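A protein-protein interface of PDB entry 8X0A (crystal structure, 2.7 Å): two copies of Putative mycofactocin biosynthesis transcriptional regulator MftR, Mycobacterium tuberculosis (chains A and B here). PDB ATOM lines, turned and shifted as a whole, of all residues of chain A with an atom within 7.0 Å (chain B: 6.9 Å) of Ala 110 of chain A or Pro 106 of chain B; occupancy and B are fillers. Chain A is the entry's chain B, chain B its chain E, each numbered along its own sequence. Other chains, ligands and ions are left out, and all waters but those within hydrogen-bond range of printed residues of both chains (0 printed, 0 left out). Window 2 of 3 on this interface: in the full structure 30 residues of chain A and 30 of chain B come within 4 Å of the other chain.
O of Thr 105 of chain A lies within hydrogen-bond range of NE2 of Gln 109 of chain A, at 3.0 Å.
O of Thr 105 of chain B sits at hydrogen-bond distance from NE2 of Gln 109 of chain B.
NE2 of Gln 109 of chain B sits at hydrogen-bond distance from O of Ile 102 of chain B, 2.9 Å away.
Pro 106 of chain A touches Ala 110 of chain B.
Met 113 of chain B touches Gln 109 of chain A.
Ala 110 of chain A touches Pro 106 of chain B (CB to O, 3.3 Å).
N of Ala 110 of chain A touches CB of Gln 109 of chain B, at 3.9 Å.
Gln 109 of chain B touches Met 113 of chain A (OE1 to CG, 3.4 Å).
Met 113 of chain A touches Met 113 of chain B.
Of chain B, only Pro 106 and Gln 109 come within 4 Å of Ala 110 of chain A.
Pro 106 of chain B touches one residue of chain A.
Printed residues of chain A within 4 Å of Met 113 of chain B: Gln 109 and Met 113.
Of the printed residues of chain B, Gln 109 of chain A touches Met 113.
Glu 107 of chain A touches none of the printed residues of chain B.
The nearest residue of chain A that does not touch Pro 106 of chain B is Gln 109 of chain A (5.7 Å).
The nearest printed residue of chain A that does not touch Met 113 of chain B is Pro 106 of chain A (6.6 Å).
Of the 11 printed residues of chain A, 4 touch a printed residue of chain B.
Hydrophobic or aromatic side chains of chain A that line the printed part of chain B: Ala 110 and Met 113.
Hydrophobic or aromatic side chains of chain B that line the printed part of chain A: Pro 106, Ala 110 and Met 113.
Along chain B the printed residues that touch a printed residue of chain A span positions 106 to 113.
Among the printed residues, 6 pairs touch across the chains.
Pro 106 of chain A touches Ala 110 of chain B, and with the chains exchanged Ala 110 of chain A touches Pro 106 of chain B.
Gln 109 of chain A touches Met 113 of chain B, and with the chains exchanged Met 113 of chain A touches Gln 109 of chain B.
Ala 110 of chain A touches Gln 109 of chain B, but with the chains exchanged Gln 109 of chain A does not touch Ala 110 of chain B (4.1 Å).
Met 113 of chain B touches its own counterpart, Met 113 of chain A.
Of the 6 pairs that touch across the chains among the printed residues, 5 have their exchanged pair printed and touching as well.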
ATOM      1  N   THR A 105     -30.259   4.992  21.179  1.00  0.00           N
ATOM      2  CA  THR A 105     -29.780   4.894  22.558  1.00  0.00           C
ATOM      3  C   THR A 105     -29.464   6.278  23.131  1.00  0.00           C
ATOM      4  O   THR A 105     -28.504   6.917  22.669  1.00  0.00           O
ATOM      5  CB  THR A 105     -28.520   4.029  22.644  1.00  0.00           C
ATOM      6  OG1 THR A 105     -28.754   2.798  21.966  1.00  0.00           O
ATOM      7  CG2 THR A 105     -28.113   3.743  24.070  1.00  0.00           C
ATOM      8  N   PRO A 106     -30.180   6.790  24.172  1.00  0.00           N
ATOM      9  CA  PRO A 106     -29.845   8.093  24.784  1.00  0.00           C
ATOM     10  C   PRO A 106     -28.382   8.341  25.186  1.00  0.00           C
ATOM     11  O   PRO A 106     -27.866   9.438  24.989  1.00  0.00           O
ATOM     12  CB  PRO A 106     -30.720   8.106  26.053  1.00  0.00           C
ATOM     13  CG  PRO A 106     -31.919   7.270  25.686  1.00  0.00           C
ATOM     14  CD  PRO A 106     -31.340   6.168  24.819  1.00  0.00           C
ATOM     15  N   GLU A 107     -27.724   7.294  25.711  1.00  0.00           N
ATOM     16  CA  GLU A 107     -26.340   7.321  26.188  1.00  0.00           C
ATOM     17  C   GLU A 107     -25.306   7.542  25.067  1.00  0.00           C
ATOM     18  O   GLU A 107     -24.175   7.916  25.382  1.00  0.00           O
ATOM     19  CB  GLU A 107     -25.996   6.014  26.901  1.00  0.00           C
ATOM     20  CG  GLU A 107     -26.671   5.835  28.264  1.00  0.00           C
ATOM     21  CD  GLU A 107     -28.106   5.331  28.290  1.00  0.00           C
ATOM     22  OE1 GLU A 107     -28.752   5.172  27.229  1.00  0.00           O
ATOM     23  OE2 GLU A 107     -28.574   5.039  29.409  1.00  0.00           O
ATOM     24  N   LEU A 108     -25.676   7.331  23.781  1.00  0.00           N
ATOM     25  CA  LEU A 108     -24.758   7.471  22.656  1.00  0.00           C
ATOM     26  C   LEU A 108     -24.802   8.857  22.016  1.00  0.00           C
ATOM     27  O   LEU A 108     -23.948   9.145  21.176  1.00  0.00           O
ATOM     28  CB  LEU A 108     -25.098   6.400  21.611  1.00  0.00           C
ATOM     29  CG  LEU A 108     -24.309   5.090  21.691  1.00  0.00           C
ATOM     30  CD1 LEU A 108     -24.171   4.551  23.095  1.00  0.00           C
ATOM     31  CD2 LEU A 108     -24.965   4.030  20.827  1.00  0.00           C
ATOM     32  N   GLN A 109     -25.772   9.694  22.400  1.00  0.00           N
ATOM     33  CA  GLN A 109     -26.082  10.913  21.660  1.00  0.00           C
ATOM     34  C   GLN A 109     -24.956  11.951  21.820  1.00  0.00           C
ATOM     35  O   GLN A 109     -24.527  12.507  20.804  1.00  0.00           O
ATOM     36  CB  GLN A 109     -27.466  11.427  22.066  1.00  0.00           C
ATOM     37  CG  GLN A 109     -28.580  10.411  21.802  1.00  0.00           C
ATOM     38  CD  GLN A 109     -28.595   9.926  20.370  1.00  0.00           C
ATOM     39  OE1 GLN A 109     -28.553  10.721  19.434  1.00  0.00           O
ATOM     40  NE2 GLN A 109     -28.525   8.621  20.184  1.00  0.00           N
ATOM     41  N   ALA A 110     -24.435  12.172  23.037  1.00  0.00           N
ATOM     42  CA  ALA A 110     -23.293  13.079  23.230  1.00  0.00           C
ATOM     43  C   ALA A 110     -22.130  12.707  22.313  1.00  0.00           C
ATOM     44  O   ALA A 110     -21.647  13.566  21.560  1.00  0.00           O
ATOM     45  CB  ALA A 110     -22.813  13.117  24.663  1.00  0.00           C
ATOM     46  N   TYR A 111     -21.750  11.416  22.336  1.00  0.00           N
ATOM     47  CA  TYR A 111     -20.635  10.914  21.537  1.00  0.00           C
ATOM     48  C   TYR A 111     -20.918  11.020  20.031  1.00  0.00           C
ATOM     49  O   TYR A 111     -20.043  11.433  19.252  1.00  0.00           O
ATOM     50  CB  TYR A 111     -20.315   9.459  21.910  1.00  0.00           C
ATOM     51  CG  TYR A 111     -19.041   9.012  21.265  1.00  0.00           C
ATOM     52  CD1 TYR A 111     -17.816   9.409  21.775  1.00  0.00           C
ATOM     53  CD2 TYR A 111     -19.044   8.252  20.108  1.00  0.00           C
ATOM     54  CE1 TYR A 111     -16.621   9.093  21.129  1.00  0.00           C
ATOM     55  CE2 TYR A 111     -17.862   7.946  19.437  1.00  0.00           C
ATOM     56  CZ  TYR A 111     -16.647   8.353  19.958  1.00  0.00           C
ATOM     57  OH  TYR A 111     -15.507   7.995  19.314  1.00  0.00           O
ATOM     58  N   SER A 112     -22.136  10.595  19.640  1.00  0.00           N
ATOM     59  CA  SER A 112     -22.644  10.703  18.279  1.00  0.00           C
ATOM     60  C   SER A 112     -22.547  12.118  17.713  1.00  0.00           C
ATOM     61  O   SER A 112     -22.196  12.252  16.532  1.00  0.00           O
ATOM     62  CB  SER A 112     -24.056  10.190  18.187  1.00  0.00           C
ATOM     63  OG  SER A 112     -24.108   8.816  18.484  1.00  0.00           O
ATOM     64  N   MET A 113     -22.855  13.157  18.530  1.00  0.00           N
ATOM     65  CA  MET A 113     -22.803  14.542  18.062  1.00  0.00           C
ATOM     66  C   MET A 113     -21.403  14.895  17.564  1.00  0.00           C
ATOM     67  O   MET A 113     -21.272  15.607  16.559  1.00  0.00           O
ATOM     68  CB  MET A 113     -23.157  15.551  19.157  1.00  0.00           C
ATOM     69  CG  MET A 113     -24.615  15.620  19.597  1.00  0.00           C
ATOM     70  SD  MET A 113     -25.931  15.419  18.332  1.00  0.00           S
ATOM     71  CE  MET A 113     -26.271  13.666  18.437  1.00  0.00           C
ATOM     72  N   THR A 114     -20.376  14.401  18.270  1.00  0.00           N
ATOM     73  CA  THR A 114     -18.974  14.575  17.891  1.00  0.00           C
ATOM     74  C   THR A 114     -18.651  13.905  16.552  1.00  0.00           C
ATOM     75  O   THR A 114     -17.851  14.441  15.779  1.00  0.00           O
ATOM     76  CB  THR A 114     -18.036  14.042  18.993  1.00  0.00           C
ATOM     77  OG1 THR A 114     -18.391  14.676  20.219  1.00  0.00           O
ATOM     78  CG2 THR A 114     -16.569  14.282  18.727  1.00  0.00           C
ATOM     79  N   MET A 115     -19.225  12.714  16.323  1.00  0.00           N
ATOM     80  CA  MET A 115     -19.008  11.974  15.079  1.00  0.00           C
ATOM     81  C   MET A 115     -19.716  12.655  13.903  1.00  0.00           C
ATOM     82  O   MET A 115     -19.139  12.792  12.831  1.00  0.00           O
ATOM     83  CB  MET A 115     -19.506  10.526  15.246  1.00  0.00           C
ATOM     84  CG  MET A 115     -18.742   9.744  16.332  1.00  0.00           C
ATOM     85  SD  MET A 115     -16.942   9.597  15.880  1.00  0.00           S
ATOM     86  CE  MET A 115     -16.221  10.753  17.043  1.00  0.00           C
ATOM     87  N   THR B  20     -22.284  21.240  34.342  1.00  0.00           N
ATOM     88  CA  THR B  20     -22.021  20.096  35.206  1.00  0.00           C
ATOM     89  C   THR B  20     -21.782  20.539  36.665  1.00  0.00           C
ATOM     90  O   THR B  20     -22.249  19.850  37.576  1.00  0.00           O
ATOM     91  CB  THR B  20     -20.971  19.157  34.550  1.00  0.00           C
ATOM     92  OG1 THR B  20     -19.756  19.880  34.318  1.00  0.00           O
ATOM     93  CG2 THR B  20     -21.358  18.510  33.229  1.00  0.00           C
ATOM     94  N   VAL B 101     -25.383  26.723  25.804  1.00  0.00           N
ATOM     95  CA  VAL B 101     -25.588  25.642  26.752  1.00  0.00           C
ATOM     96  C   VAL B 101     -26.221  24.443  26.032  1.00  0.00           C
ATOM     97  O   VAL B 101     -25.726  23.328  26.166  1.00  0.00           O
ATOM     98  CB  VAL B 101     -26.429  26.120  27.956  1.00  0.00           C
ATOM     99  CG1 VAL B 101     -27.041  24.976  28.766  1.00  0.00           C
ATOM    100  CG2 VAL B 101     -25.647  27.094  28.840  1.00  0.00           C
ATOM    101  N   ILE B 102     -27.302  24.656  25.266  1.00  0.00           N
ATOM    102  CA  ILE B 102     -28.040  23.560  24.653  1.00  0.00           C
ATOM    103  C   ILE B 102     -27.156  22.852  23.630  1.00  0.00           C
ATOM    104  O   ILE B 102     -27.034  21.631  23.671  1.00  0.00           O
ATOM    105  CB  ILE B 102     -29.383  24.031  24.073  1.00  0.00           C
ATOM    106  CG1 ILE B 102     -30.353  24.379  25.211  1.00  0.00           C
ATOM    107  CG2 ILE B 102     -29.968  22.977  23.138  1.00  0.00           C
ATOM    108  CD1 ILE B 102     -31.698  24.964  24.774  1.00  0.00           C
ATOM    109  N   LEU B 103     -26.547  23.608  22.720  1.00  0.00           N
ATOM    110  CA  LEU B 103     -25.804  23.029  21.606  1.00  0.00           C
ATOM    111  C   LEU B 103     -24.478  22.410  22.044  1.00  0.00           C
ATOM    112  O   LEU B 103     -24.093  21.406  21.471  1.00  0.00           O
ATOM    113  CB  LEU B 103     -25.589  24.087  20.514  1.00  0.00           C
ATOM    114  CG  LEU B 103     -26.865  24.553  19.815  1.00  0.00           C
ATOM    115  CD1 LEU B 103     -26.570  25.643  18.807  1.00  0.00           C
ATOM    116  CD2 LEU B 103     -27.579  23.387  19.140  1.00  0.00           C
ATOM    117  N   GLN B 104     -23.808  22.969  23.053  1.00  0.00           N
ATOM    118  CA  GLN B 104     -22.423  22.623  23.346  1.00  0.00           C
ATOM    119  C   GLN B 104     -22.291  21.709  24.574  1.00  0.00           C
ATOM    120  O   GLN B 104     -21.225  21.123  24.693  1.00  0.00           O
ATOM    121  CB  GLN B 104     -21.580  23.888  23.484  1.00  0.00           C
ATOM    122  CG  GLN B 104     -21.656  24.816  22.278  1.00  0.00           C
ATOM    123  CD  GLN B 104     -20.902  26.137  22.431  1.00  0.00           C
ATOM    124  OE1 GLN B 104     -20.844  26.962  21.514  1.00  0.00           O
ATOM    125  NE2 GLN B 104     -20.319  26.386  23.598  1.00  0.00           N
ATOM    126  N   THR B 105     -23.324  21.491  25.412  1.00  0.00           N
ATOM    127  CA  THR B 105     -23.213  20.666  26.621  1.00  0.00           C
ATOM    128  C   THR B 105     -23.441  19.176  26.325  1.00  0.00           C
ATOM    129  O   THR B 105     -24.575  18.790  26.039  1.00  0.00           O
ATOM    130  CB  THR B 105     -24.272  21.097  27.659  1.00  0.00           C
ATOM    131  OG1 THR B 105     -24.077  22.483  27.911  1.00  0.00           O
ATOM    132  CG2 THR B 105     -24.195  20.363  28.973  1.00  0.00           C
ATOM    133  N   PRO B 106     -22.434  18.272  26.452  1.00  0.00           N
ATOM    134  CA  PRO B 106     -22.643  16.829  26.227  1.00  0.00           C
ATOM    135  C   PRO B 106     -23.808  16.159  26.967  1.00  0.00           C
ATOM    136  O   PRO B 106     -24.524  15.332  26.390  1.00  0.00           O
ATOM    137  CB  PRO B 106     -21.324  16.208  26.717  1.00  0.00           C
ATOM    138  CG  PRO B 106     -20.302  17.273  26.392  1.00  0.00           C
ATOM    139  CD  PRO B 106     -21.019  18.557  26.758  1.00  0.00           C
ATOM    140  N   GLU B 107     -24.029  16.580  28.220  1.00  0.00           N
ATOM    141  CA  GLU B 107     -25.024  16.001  29.119  1.00  0.00           C
ATOM    142  C   GLU B 107     -26.458  16.358  28.714  1.00  0.00           C
ATOM    143  O   GLU B 107     -27.390  15.703  29.185  1.00  0.00           O
ATOM    144  CB  GLU B 107     -24.759  16.401  30.578  1.00  0.00           C
ATOM    145  CG  GLU B 107     -23.443  15.853  31.161  1.00  0.00           C
ATOM    146  CD  GLU B 107     -22.123  16.513  30.732  1.00  0.00           C
ATOM    147  OE1 GLU B 107     -22.178  17.616  30.092  1.00  0.00           O
ATOM    148  OE2 GLU B 107     -21.055  15.885  30.910  1.00  0.00           O
ATOM    149  N   LEU B 108     -26.647  17.377  27.860  1.00  0.00           N
ATOM    150  CA  LEU B 108     -27.963  17.825  27.409  1.00  0.00           C
ATOM    151  C   LEU B 108     -28.417  17.169  26.108  1.00  0.00           C
ATOM    152  O   LEU B 108     -29.576  17.355  25.726  1.00  0.00           O
ATOM    153  CB  LEU B 108     -27.926  19.343  27.207  1.00  0.00           C
ATOM    154  CG  LEU B 108     -28.110  20.152  28.467  1.00  0.00           C
ATOM    155  CD1 LEU B 108     -28.047  21.640  28.126  1.00  0.00           C
ATOM    156  CD2 LEU B 108     -29.443  19.789  29.134  1.00  0.00           C
ATOM    157  N   GLN B 109     -27.535  16.415  25.443  1.00  0.00           N
ATOM    158  CA  GLN B 109     -27.760  15.977  24.077  1.00  0.00           C
ATOM    159  C   GLN B 109     -28.858  14.918  24.035  1.00  0.00           C
ATOM    160  O   GLN B 109     -29.745  15.056  23.194  1.00  0.00           O
ATOM    161  CB  GLN B 109     -26.442  15.515  23.449  1.00  0.00           C
ATOM    162  CG  GLN B 109     -25.408  16.635  23.378  1.00  0.00           C
ATOM    163  CD  GLN B 109     -25.952  17.859  22.678  1.00  0.00           C
ATOM    164  OE1 GLN B 109     -26.447  17.753  21.562  1.00  0.00           O
ATOM    165  NE2 GLN B 109     -25.924  19.002  23.352  1.00  0.00           N
ATOM    166  N   ALA B 110     -28.845  13.927  24.950  1.00  0.00           N
ATOM    167  CA  ALA B 110     -29.913  12.941  25.014  1.00  0.00           C
ATOM    168  C   ALA B 110     -31.294  13.621  25.083  1.00  0.00           C
ATOM    169  O   ALA B 110     -32.175  13.331  24.267  1.00  0.00           O
ATOM    170  CB  ALA B 110     -29.673  12.034  26.186  1.00  0.00           C
ATOM    171  N   MET B 113     -32.271  15.679  21.949  1.00  0.00           N
ATOM    172  CA  MET B 113     -32.723  14.866  20.834  1.00  0.00           C
ATOM    173  C   MET B 113     -34.242  14.664  20.884  1.00  0.00           C
ATOM    174  O   MET B 113     -34.894  14.664  19.831  1.00  0.00           O
ATOM    175  CB  MET B 113     -32.080  13.471  20.835  1.00  0.00           C
ATOM    176  CG  MET B 113     -30.596  13.376  20.478  1.00  0.00           C
ATOM    177  SD  MET B 113     -29.931  14.476  19.172  1.00  0.00           S
ATOM    178  CE  MET B 113     -29.326  15.833  20.151  1.00  0.00           C
